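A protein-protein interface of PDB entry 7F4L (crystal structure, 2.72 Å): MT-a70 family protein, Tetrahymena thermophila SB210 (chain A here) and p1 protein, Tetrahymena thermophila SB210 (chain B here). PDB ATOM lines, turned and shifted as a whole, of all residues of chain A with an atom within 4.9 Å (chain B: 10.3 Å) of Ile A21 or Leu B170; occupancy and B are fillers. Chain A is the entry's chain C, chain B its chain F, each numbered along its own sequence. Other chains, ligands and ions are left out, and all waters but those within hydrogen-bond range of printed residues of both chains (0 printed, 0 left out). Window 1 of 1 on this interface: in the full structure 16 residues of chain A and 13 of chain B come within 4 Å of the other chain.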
ATOM      1  N   LEU A  17     -18.506   6.380  -9.667  1.00  0.00           N
ATOM      2  CA  LEU A  17     -18.753   5.642  -8.444  1.00  0.00           C
ATOM      3  C   LEU A  17     -19.937   6.219  -7.703  1.00  0.00           C
ATOM      4  O   LEU A  17     -20.734   5.482  -7.123  1.00  0.00           O
ATOM      5  CB  LEU A  17     -17.525   5.676  -7.550  1.00  0.00           C
ATOM      6  CG  LEU A  17     -17.123   4.411  -6.843  1.00  0.00           C
ATOM      7  CD1 LEU A  17     -16.394   4.815  -5.663  1.00  0.00           C
ATOM      8  CD2 LEU A  17     -18.316   3.577  -6.476  1.00  0.00           C
ATOM      9  N   LEU A  18     -20.055   7.537  -7.683  1.00  0.00           N
ATOM     10  CA  LEU A  18     -21.190   8.107  -6.994  1.00  0.00           C
ATOM     11  C   LEU A  18     -22.470   7.757  -7.719  1.00  0.00           C
ATOM     12  O   LEU A  18     -23.489   7.469  -7.089  1.00  0.00           O
ATOM     13  CB  LEU A  18     -21.018   9.614  -6.867  1.00  0.00           C
ATOM     14  CG  LEU A  18     -22.173  10.379  -6.245  1.00  0.00           C
ATOM     15  CD1 LEU A  18     -22.193  10.077  -4.787  1.00  0.00           C
ATOM     16  CD2 LEU A  18     -21.974  11.843  -6.469  1.00  0.00           C
ATOM     17  N   GLN A  19     -22.428   7.724  -9.038  1.00  0.00           N
ATOM     18  CA  GLN A  19     -23.613   7.353  -9.779  1.00  0.00           C
ATOM     19  C   GLN A  19     -24.004   5.930  -9.464  1.00  0.00           C
ATOM     20  O   GLN A  19     -25.170   5.655  -9.191  1.00  0.00           O
ATOM     21  CB  GLN A  19     -23.349   7.535 -11.263  1.00  0.00           C
ATOM     22  CG  GLN A  19     -24.548   7.899 -12.093  1.00  0.00           C
ATOM     23  CD  GLN A  19     -24.369   7.475 -13.522  1.00  0.00           C
ATOM     24  OE1 GLN A  19     -24.502   6.295 -13.848  1.00  0.00           O
ATOM     25  NE2 GLN A  19     -24.035   8.427 -14.385  1.00  0.00           N
ATOM     26  N   ASP A  20     -23.032   5.017  -9.453  1.00  0.00           N
ATOM     27  CA  ASP A  20     -23.319   3.613  -9.164  1.00  0.00           C
ATOM     28  C   ASP A  20     -23.733   3.390  -7.711  1.00  0.00           C
ATOM     29  O   ASP A  20     -24.503   2.474  -7.424  1.00  0.00           O
ATOM     30  CB  ASP A  20     -22.102   2.752  -9.504  1.00  0.00           C
ATOM     31  CG  ASP A  20     -22.002   2.433 -10.992  1.00  0.00           C
ATOM     32  OD1 ASP A  20     -22.748   3.030 -11.788  1.00  0.00           O
ATOM     33  OD2 ASP A  20     -21.154   1.604 -11.381  1.00  0.00           O
ATOM     34  N   ILE A  21     -23.229   4.195  -6.781  1.00  0.00           N
ATOM     35  CA  ILE A  21     -23.646   4.046  -5.394  1.00  0.00           C
ATOM     36  C   ILE A  21     -25.103   4.415  -5.243  1.00  0.00           C
ATOM     37  O   ILE A  21     -25.835   3.794  -4.469  1.00  0.00           O
ATOM     38  CB  ILE A  21     -22.761   4.905  -4.478  1.00  0.00           C
ATOM     39  CG1 ILE A  21     -21.372   4.326  -4.413  1.00  0.00           C
ATOM     40  CG2 ILE A  21     -23.302   4.964  -3.092  1.00  0.00           C
ATOM     41  CD1 ILE A  21     -20.472   5.215  -3.733  1.00  0.00           C
ATOM     42  N   GLU A  22     -25.545   5.414  -5.999  1.00  0.00           N
ATOM     43  CA  GLU A  22     -26.909   5.900  -5.914  1.00  0.00           C
ATOM     44  C   GLU A  22     -27.903   4.857  -6.381  1.00  0.00           C
ATOM     45  O   GLU A  22     -28.887   4.584  -5.691  1.00  0.00           O
ATOM     46  CB  GLU A  22     -27.045   7.168  -6.743  1.00  0.00           C
ATOM     47  CG  GLU A  22     -27.946   8.171  -6.125  1.00  0.00           C
ATOM     48  CD  GLU A  22     -27.367   8.762  -4.878  1.00  0.00           C
ATOM     49  OE1 GLU A  22     -26.311   9.416  -4.999  1.00  0.00           O
ATOM     50  OE2 GLU A  22     -27.960   8.564  -3.790  1.00  0.00           O
ATOM     51  N   LYS A  23     -27.685   4.285  -7.566  1.00  0.00           N
ATOM     52  CA  LYS A  23     -28.554   3.213  -8.035  1.00  0.00           C
ATOM     53  C   LYS A  23     -28.604   2.080  -7.026  1.00  0.00           C
ATOM     54  O   LYS A  23     -29.659   1.502  -6.759  1.00  0.00           O
ATOM     55  CB  LYS A  23     -28.066   2.677  -9.382  1.00  0.00           C
ATOM     56  CG  LYS A  23     -27.923   3.706 -10.500  1.00  0.00           C
ATOM     57  CD  LYS A  23     -27.335   3.102 -11.786  1.00  0.00           C
ATOM     58  CE  LYS A  23     -27.271   4.152 -12.898  1.00  0.00           C
ATOM     59  NZ  LYS A  23     -26.312   3.847 -14.009  1.00  0.00           N
ATOM     60  N   ARG A  24     -27.458   1.739  -6.469  1.00  0.00           N
ATOM     61  CA  ARG A  24     -27.366   0.654  -5.509  1.00  0.00           C
ATOM     62  C   ARG A  24     -28.136   0.929  -4.246  1.00  0.00           C
ATOM     63  O   ARG A  24     -28.665   0.029  -3.634  1.00  0.00           O
ATOM     64  CB  ARG A  24     -25.920   0.315  -5.201  1.00  0.00           C
ATOM     65  CG  ARG A  24     -25.234  -0.382  -6.342  1.00  0.00           C
ATOM     66  CD  ARG A  24     -25.240  -1.871  -6.129  1.00  0.00           C
ATOM     67  NE  ARG A  24     -26.307  -2.543  -6.846  1.00  0.00           N
ATOM     68  CZ  ARG A  24     -26.602  -3.819  -6.684  1.00  0.00           C
ATOM     69  NH1 ARG A  24     -25.911  -4.540  -5.841  1.00  0.00           N
ATOM     70  NH2 ARG A  24     -27.582  -4.374  -7.362  1.00  0.00           N
ATOM     71  N   ILE A  25     -28.141   2.180  -3.821  1.00  0.00           N
ATOM     72  CA  ILE A  25     -28.881   2.530  -2.624  1.00  0.00           C
ATOM     73  C   ILE A  25     -30.359   2.351  -2.865  1.00  0.00           C
ATOM     74  O   ILE A  25     -31.078   1.822  -2.020  1.00  0.00           O
ATOM     75  CB  ILE A  25     -28.551   3.963  -2.181  1.00  0.00           C
ATOM     76  CG1 ILE A  25     -27.280   3.987  -1.332  1.00  0.00           C
ATOM     77  CG2 ILE A  25     -29.694   4.543  -1.409  1.00  0.00           C
ATOM     78  CD1 ILE A  25     -26.787   5.343  -1.076  1.00  0.00           C
ATOM     79  N   TYR A  28     -31.089  -1.452  -2.706  1.00  0.00           N
ATOM     80  CA  TYR A  28     -31.179  -2.041  -1.375  1.00  0.00           C
ATOM     81  C   TYR A  28     -32.242  -1.396  -0.513  1.00  0.00           C
ATOM     82  O   TYR A  28     -32.677  -2.001   0.467  1.00  0.00           O
ATOM     83  CB  TYR A  28     -29.838  -1.958  -0.665  1.00  0.00           C
ATOM     84  CG  TYR A  28     -28.888  -2.961  -1.206  1.00  0.00           C
ATOM     85  CD1 TYR A  28     -29.018  -4.290  -0.886  1.00  0.00           C
ATOM     86  CD2 TYR A  28     -27.913  -2.593  -2.102  1.00  0.00           C
ATOM     87  CE1 TYR A  28     -28.175  -5.215  -1.412  1.00  0.00           C
ATOM     88  CE2 TYR A  28     -27.071  -3.504  -2.627  1.00  0.00           C
ATOM     89  CZ  TYR A  28     -27.201  -4.812  -2.282  1.00  0.00           C
ATOM     90  OH  TYR A  28     -26.332  -5.720  -2.815  1.00  0.00           O
ATOM     91  N   PHE B 161     -23.903  -9.909   4.953  1.00  0.00           N
ATOM     92  CA  PHE B 161     -24.345  -8.604   5.388  1.00  0.00           C
ATOM     93  C   PHE B 161     -25.846  -8.532   5.355  1.00  0.00           C
ATOM     94  O   PHE B 161     -26.457  -9.153   4.528  1.00  0.00           O
ATOM     95  CB  PHE B 161     -23.829  -7.571   4.406  1.00  0.00           C
ATOM     96  CG  PHE B 161     -22.431  -7.151   4.652  1.00  0.00           C
ATOM     97  CD1 PHE B 161     -21.994  -6.894   5.928  1.00  0.00           C
ATOM     98  CD2 PHE B 161     -21.553  -7.009   3.610  1.00  0.00           C
ATOM     99  CE1 PHE B 161     -20.698  -6.503   6.158  1.00  0.00           C
ATOM    100  CE2 PHE B 161     -20.261  -6.612   3.828  1.00  0.00           C
ATOM    101  CZ  PHE B 161     -19.832  -6.358   5.101  1.00  0.00           C
ATOM    102  N   THR B 162     -26.453  -7.741   6.221  1.00  0.00           N
ATOM    103  CA  THR B 162     -27.885  -7.547   6.091  1.00  0.00           C
ATOM    104  C   THR B 162     -28.165  -6.309   5.256  1.00  0.00           C
ATOM    105  O   THR B 162     -27.282  -5.505   4.966  1.00  0.00           O
ATOM    106  CB  THR B 162     -28.539  -7.425   7.463  1.00  0.00           C
ATOM    107  OG1 THR B 162     -28.494  -6.067   7.895  1.00  0.00           O
ATOM    108  CG2 THR B 162     -27.784  -8.224   8.444  1.00  0.00           C
ATOM    109  N   ASN B 163     -29.422  -6.164   4.859  1.00  0.00           N
ATOM    110  CA  ASN B 163     -29.805  -5.017   4.050  1.00  0.00           C
ATOM    111  C   ASN B 163     -29.400  -3.715   4.710  1.00  0.00           C
ATOM    112  O   ASN B 163     -28.968  -2.784   4.036  1.00  0.00           O
ATOM    113  CB  ASN B 163     -31.301  -5.036   3.804  1.00  0.00           C
ATOM    114  CG  ASN B 163     -31.699  -6.057   2.801  1.00  0.00           C
ATOM    115  OD1 ASN B 163     -31.073  -6.198   1.768  1.00  0.00           O
ATOM    116  ND2 ASN B 163     -32.736  -6.809   3.115  1.00  0.00           N
ATOM    117  N   LEU B 164     -29.530  -3.634   6.026  1.00  0.00           N
ATOM    118  CA  LEU B 164     -29.222  -2.411   6.743  1.00  0.00           C
ATOM    119  C   LEU B 164     -27.736  -2.185   6.846  1.00  0.00           C
ATOM    120  O   LEU B 164     -27.288  -1.048   6.791  1.00  0.00           O
ATOM    121  CB  LEU B 164     -29.810  -2.461   8.146  1.00  0.00           C
ATOM    122  CG  LEU B 164     -30.342  -1.242   8.904  1.00  0.00           C
ATOM    123  CD1 LEU B 164     -30.267  -1.521  10.340  1.00  0.00           C
ATOM    124  CD2 LEU B 164     -29.650   0.034   8.608  1.00  0.00           C
ATOM    125  N   GLU B 165     -26.961  -3.239   7.021  1.00  0.00           N
ATOM    126  CA  GLU B 165     -25.515  -3.079   7.030  1.00  0.00           C
ATOM    127  C   GLU B 165     -25.010  -2.630   5.667  1.00  0.00           C
ATOM    128  O   GLU B 165     -24.152  -1.752   5.571  1.00  0.00           O
ATOM    129  CB  GLU B 165     -24.856  -4.388   7.453  1.00  0.00           C
ATOM    130  CG  GLU B 165     -25.332  -4.883   8.779  1.00  0.00           C
ATOM    131  CD  GLU B 165     -24.763  -6.215   9.124  1.00  0.00           C
ATOM    132  OE1 GLU B 165     -24.749  -7.099   8.250  1.00  0.00           O
ATOM    133  OE2 GLU B 165     -24.338  -6.392  10.277  1.00  0.00           O
ATOM    134  N   ILE B 166     -25.529  -3.225   4.604  1.00  0.00           N
ATOM    135  CA  ILE B 166     -25.125  -2.811   3.273  1.00  0.00           C
ATOM    136  C   ILE B 166     -25.406  -1.334   3.081  1.00  0.00           C
ATOM    137  O   ILE B 166     -24.531  -0.568   2.676  1.00  0.00           O
ATOM    138  CB  ILE B 166     -25.843  -3.664   2.221  1.00  0.00           C
ATOM    139  CG1 ILE B 166     -25.442  -5.123   2.355  1.00  0.00           C
ATOM    140  CG2 ILE B 166     -25.546  -3.147   0.862  1.00  0.00           C
ATOM    141  CD1 ILE B 166     -26.270  -6.022   1.554  1.00  0.00           C
ATOM    142  N   LEU B 167     -26.631  -0.910   3.392  1.00  0.00           N
ATOM    143  CA  LEU B 167     -27.005   0.489   3.242  1.00  0.00           C
ATOM    144  C   LEU B 167     -26.132   1.413   4.073  1.00  0.00           C
ATOM    145  O   LEU B 167     -25.800   2.511   3.622  1.00  0.00           O
ATOM    146  CB  LEU B 167     -28.463   0.678   3.603  1.00  0.00           C
ATOM    147  CG  LEU B 167     -29.387   0.168   2.510  1.00  0.00           C
ATOM    148  CD1 LEU B 167     -30.725  -0.119   3.056  1.00  0.00           C
ATOM    149  CD2 LEU B 167     -29.497   1.160   1.410  1.00  0.00           C
ATOM    150  N   THR B 168     -25.734   0.989   5.266  1.00  0.00           N
ATOM    151  CA  THR B 168     -24.830   1.804   6.066  1.00  0.00           C
ATOM    152  C   THR B 168     -23.471   1.962   5.390  1.00  0.00           C
ATOM    153  O   THR B 168     -22.922   3.064   5.347  1.00  0.00           O
ATOM    154  CB  THR B 168     -24.680   1.204   7.460  1.00  0.00           C
ATOM    155  OG1 THR B 168     -25.963   0.971   8.028  1.00  0.00           O
ATOM    156  CG2 THR B 168     -23.955   2.132   8.331  1.00  0.00           C
ATOM    157  N   HIS B 169     -22.911   0.870   4.858  1.00  0.00           N
ATOM    158  CA  HIS B 169     -21.683   0.953   4.071  1.00  0.00           C
ATOM    159  C   HIS B 169     -21.849   1.872   2.879  1.00  0.00           C
ATOM    160  O   HIS B 169     -21.007   2.729   2.622  1.00  0.00           O
ATOM    161  CB  HIS B 169     -21.263  -0.424   3.587  1.00  0.00           C
ATOM    162  CG  HIS B 169     -20.578  -1.237   4.628  1.00  0.00           C
ATOM    163  ND1 HIS B 169     -19.476  -0.783   5.313  1.00  0.00           N
ATOM    164  CD2 HIS B 169     -20.860  -2.455   5.134  1.00  0.00           C
ATOM    165  CE1 HIS B 169     -19.097  -1.691   6.188  1.00  0.00           C
ATOM    166  NE2 HIS B 169     -19.928  -2.713   6.104  1.00  0.00           N
ATOM    167  N   LEU B 170     -22.921   1.693   2.120  1.00  0.00           N
ATOM    168  CA  LEU B 170     -23.160   2.559   0.974  1.00  0.00           C
ATOM    169  C   LEU B 170     -23.269   4.015   1.393  1.00  0.00           C
ATOM    170  O   LEU B 170     -22.708   4.903   0.751  1.00  0.00           O
ATOM    171  CB  LEU B 170     -24.417   2.125   0.255  1.00  0.00           C
ATOM    172  CG  LEU B 170     -24.440   0.761  -0.394  1.00  0.00           C
ATOM    173  CD1 LEU B 170     -25.833   0.478  -0.835  1.00  0.00           C
ATOM    174  CD2 LEU B 170     -23.522   0.772  -1.561  1.00  0.00           C
ATOM    175  N   TYR B 171     -24.006   4.293   2.457  1.00  0.00           N
ATOM    176  CA  TYR B 171     -24.104   5.674   2.899  1.00  0.00           C
ATOM    177  C   TYR B 171     -22.749   6.214   3.328  1.00  0.00           C
ATOM    178  O   TYR B 171     -22.380   7.330   2.963  1.00  0.00           O
ATOM    179  CB  TYR B 171     -25.123   5.796   4.016  1.00  0.00           C
ATOM    180  CG  TYR B 171     -26.490   6.095   3.489  1.00  0.00           C
ATOM    181  CD1 TYR B 171     -26.982   7.370   3.485  1.00  0.00           C
ATOM    182  CD2 TYR B 171     -27.277   5.103   2.966  1.00  0.00           C
ATOM    183  CE1 TYR B 171     -28.209   7.640   2.998  1.00  0.00           C
ATOM    184  CE2 TYR B 171     -28.513   5.372   2.478  1.00  0.00           C
ATOM    185  CZ  TYR B 171     -28.967   6.642   2.496  1.00  0.00           C
ATOM    186  OH  TYR B 171     -30.205   6.918   2.007  1.00  0.00           O
ATOM    187  N   ASN B 172     -21.980   5.432   4.083  1.00  0.00           N
ATOM    188  CA  ASN B 172     -20.656   5.886   4.487  1.00  0.00           C
ATOM    189  C   ASN B 172     -19.781   6.151   3.284  1.00  0.00           C
ATOM    190  O   ASN B 172     -19.058   7.147   3.227  1.00  0.00           O
ATOM    191  CB  ASN B 172     -19.988   4.852   5.374  1.00  0.00           C
ATOM    192  CG  ASN B 172     -20.644   4.721   6.699  1.00  0.00           C
ATOM    193  OD1 ASN B 172     -21.298   5.634   7.179  1.00  0.00           O
ATOM    194  ND2 ASN B 172     -20.458   3.581   7.318  1.00  0.00           N
ATOM    195  N   LEU B 173     -19.812   5.240   2.323  1.00  0.00           N
ATOM    196  CA  LEU B 173     -19.061   5.406   1.093  1.00  0.00           C
ATOM    197  C   LEU B 173     -19.419   6.718   0.426  1.00  0.00           C
ATOM    198  O   LEU B 173     -18.564   7.566   0.172  1.00  0.00           O
ATOM    199  CB  LEU B 173     -19.367   4.240   0.175  1.00  0.00           C
ATOM    200  CG  LEU B 173     -18.238   3.497  -0.503  1.00  0.00           C
ATOM    201  CD1 LEU B 173     -18.808   2.928  -1.721  1.00  0.00           C
ATOM    202  CD2 LEU B 173     -17.075   4.378  -0.842  1.00  0.00           C
ATOM    203  N   LYS B 174     -20.702   6.897   0.160  1.00  0.00           N
ATOM    204  CA  LYS B 174     -21.178   8.105  -0.488  1.00  0.00           C
ATOM    205  C   LYS B 174     -20.600   9.354   0.153  1.00  0.00           C
ATOM    206  O   LYS B 174     -20.096  10.239  -0.539  1.00  0.00           O
ATOM    207  CB  LYS B 174     -22.698   8.128  -0.441  1.00  0.00           C
ATOM    208  CG  LYS B 174     -23.292   9.275  -1.170  1.00  0.00           C
ATOM    209  CD  LYS B 174     -24.699   9.509  -0.745  1.00  0.00           C
ATOM    210  CE  LYS B 174     -25.501  10.114  -1.858  1.00  0.00           C
ATOM    211  NZ  LYS B 174     -26.445  11.120  -1.329  1.00  0.00           N
ATOM    212  N   ALA B 175     -20.638   9.435   1.476  1.00  0.00           N
ATOM    213  CA  ALA B 175     -20.089  10.609   2.143  1.00  0.00           C
ATOM    214  C   ALA B 175     -18.638  10.836   1.751  1.00  0.00           C
ATOM    215  O   ALA B 175     -18.263  11.927   1.307  1.00  0.00           O
ATOM    216  CB  ALA B 175     -20.214  10.457   3.653  1.00  0.00           C
ATOM    217  N   GLU B 176     -17.813   9.804   1.894  1.00  0.00           N
ATOM    218  CA  GLU B 176     -16.404   9.919   1.559  1.00  0.00           C
ATOM    219  C   GLU B 176     -16.211  10.408   0.145  1.00  0.00           C
ATOM    220  O   GLU B 176     -15.417  11.311  -0.104  1.00  0.00           O
ATOM    221  CB  GLU B 176     -15.711   8.586   1.721  1.00  0.00           C
ATOM    222  CG  GLU B 176     -14.612   8.651   2.726  1.00  0.00           C
ATOM    223  CD  GLU B 176     -13.488   9.536   2.291  1.00  0.00           C
ATOM    224  OE1 GLU B 176     -13.313   9.732   1.085  1.00  0.00           O
ATOM    225  OE2 GLU B 176     -12.761  10.038   3.155  1.00  0.00           O
ATOM    226  N   ILE B 177     -16.933   9.830  -0.796  1.00  0.00           N
ATOM    227  CA  ILE B 177     -16.871  10.331  -2.157  1.00  0.00           C
ATOM    228  C   ILE B 177     -17.253  11.797  -2.207  1.00  0.00           C
ATOM    229  O   ILE B 177     -16.424  12.660  -2.515  1.00  0.00           O
ATOM    230  CB  ILE B 177     -17.774   9.505  -3.065  1.00  0.00           C
ATOM    231  CG1 ILE B 177     -17.254   8.109  -3.073  1.00  0.00           C
ATOM    232  CG2 ILE B 177     -17.774  10.078  -4.440  1.00  0.00           C
ATOM    233  CD1 ILE B 177     -17.934   7.370  -4.052  1.00  0.00           C
ATOM    234  N   VAL B 178     -18.517  12.093  -1.916  1.00  0.00           N
ATOM    235  CA  VAL B 178     -19.019  13.452  -1.921  1.00  0.00           C
ATOM    236  C   VAL B 178     -17.996  14.381  -1.298  1.00  0.00           C
ATOM    237  O   VAL B 178     -17.784  15.492  -1.785  1.00  0.00           O
ATOM    238  CB  VAL B 178     -20.353  13.534  -1.184  1.00  0.00           C
ATOM    239  CG1 VAL B 178     -20.778  14.952  -1.090  1.00  0.00           C
ATOM    240  CG2 VAL B 178     -21.378  12.757  -1.934  1.00  0.00           C
ATOM    241  N   ARG B 179     -17.317  13.920  -0.253  1.00  0.00           N
ATOM    242  CA  ARG B 179     -16.290  14.744   0.350  1.00  0.00           C
ATOM    243  C   ARG B 179     -15.016  14.771  -0.479  1.00  0.00           C
ATOM    244  O   ARG B 179     -14.273  15.748  -0.409  1.00  0.00           O
ATOM    245  CB  ARG B 179     -16.001  14.265   1.773  1.00  0.00           C
ATOM    246  CG  ARG B 179     -14.884  15.000   2.501  1.00  0.00           C
ATOM    247  CD  ARG B 179     -13.559  14.197   2.481  1.00  0.00           C
ATOM    248  NE  ARG B 179     -13.250  13.680   3.785  1.00  0.00           N
ATOM    249  CZ  ARG B 179     -12.206  12.898   4.028  1.00  0.00           C
ATOM    250  NH1 ARG B 179     -11.408  12.555   3.026  1.00  0.00           N
ATOM    251  NH2 ARG B 179     -11.950  12.437   5.268  1.00  0.00           N
ATOM    252  N   LEU B 181     -15.230  14.703  -3.783  1.00  0.00           N
ATOM    253  CA  LEU B 181     -15.690  15.667  -4.761  1.00  0.00           C
ATOM    254  C   LEU B 181     -15.707  17.068  -4.167  1.00  0.00           C
ATOM    255  O   LEU B 181     -15.467  18.050  -4.875  1.00  0.00           O
ATOM    256  CB  LEU B 181     -17.064  15.265  -5.262  1.00  0.00           C
ATOM    257  CG  LEU B 181     -17.085  13.924  -5.973  1.00  0.00           C
ATOM    258  CD1 LEU B 181     -18.450  13.564  -6.456  1.00  0.00           C
ATOM    259  CD2 LEU B 181     -16.172  13.959  -7.143  1.00  0.00           C
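Ile A21 touches just these residues of chain B: Leu B170, Leu B173 and Ile B177. Of the printed residues of chain A, Leu B170 touches Ile A21 (3.9 Å), Ile A25 (3.8 Å) and Tyr A28 (3.9 Å). Leu A17 touches just one residue of chain B: Ile B177. Asp A20 touches none of the printed residues of chain B. Glu A22 touches just one residue of chain B: Lys B174. Of the printed residues of chain A, Lys B174 touches Leu A18 (3.9 Å) and Glu A22 (3.3 Å). Of the printed residues of chain A, Ile B166 touches Tyr A28 (3.6 Å). Of the printed residues of chain B, Tyr A28 touches Asn B163 (3.9 Å), Ile B166 (3.6 Å), Leu B167 (3.7 Å) and Leu B170 (3.9 Å). The nearest residue of chain B that does not touch Ile A21 is Lys B174 (4.2 Å). The nearest printed residue of chain A that does not touch Leu B170 is Arg A24 (4.01 Å).
CG of Lys B174 touches CD1 of Leu A18, at 3.9 Å. Leu B181 touches Leu A18. Ile A21 touches Leu B170 (CG2 to O, 3.9 Å). CD1 of Leu B173 touches CD1 of Ile A21, at 3.5 Å. Ile B177 touches Ile A21 (CD1 to CD1, 3.3 Å). Leu B167 touches Ile A25 (CD2 to O, 3.8 Å). CB of Leu B170 touches CG1 of Ile A25, at 3.8 Å. CD1 of Ile A25 touches CE2 of Tyr B171, at 3.95 Å. CE1 of Tyr A28 touches CD1 of Ile B166, 3.6 Å away. Tyr A28 touches Leu B167.
NH1 of Arg A24 sits at hydrogen-bond distance from OH of Tyr A28 (3.3 Å).
Printed residues of chain B that touch a printed residue of chain A: Asn B163, Ile B166, Leu B167, Leu B170, Tyr B171, Leu B173, Lys B174, Ile B177, Val B178 and Leu B181. Hydrophobic or aromatic side chains of chain B within 4 Å of the printed part of chain A: Ile B166, Leu B167, Leu B170, Tyr B171, Leu B173, Ile B177, Val B178 and Leu B181. Of the 10 printed residues of chain A, 6 touch a printed residue of chain B. Hydrophobic or aromatic side chains of chain A within 4 Å of the printed part of chain B: Leu A17, Leu A18, Ile A21, Ile A25 and Tyr A28.
OE2 of Glu A22 is in salt-bridge range of NZ of Lys B174.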
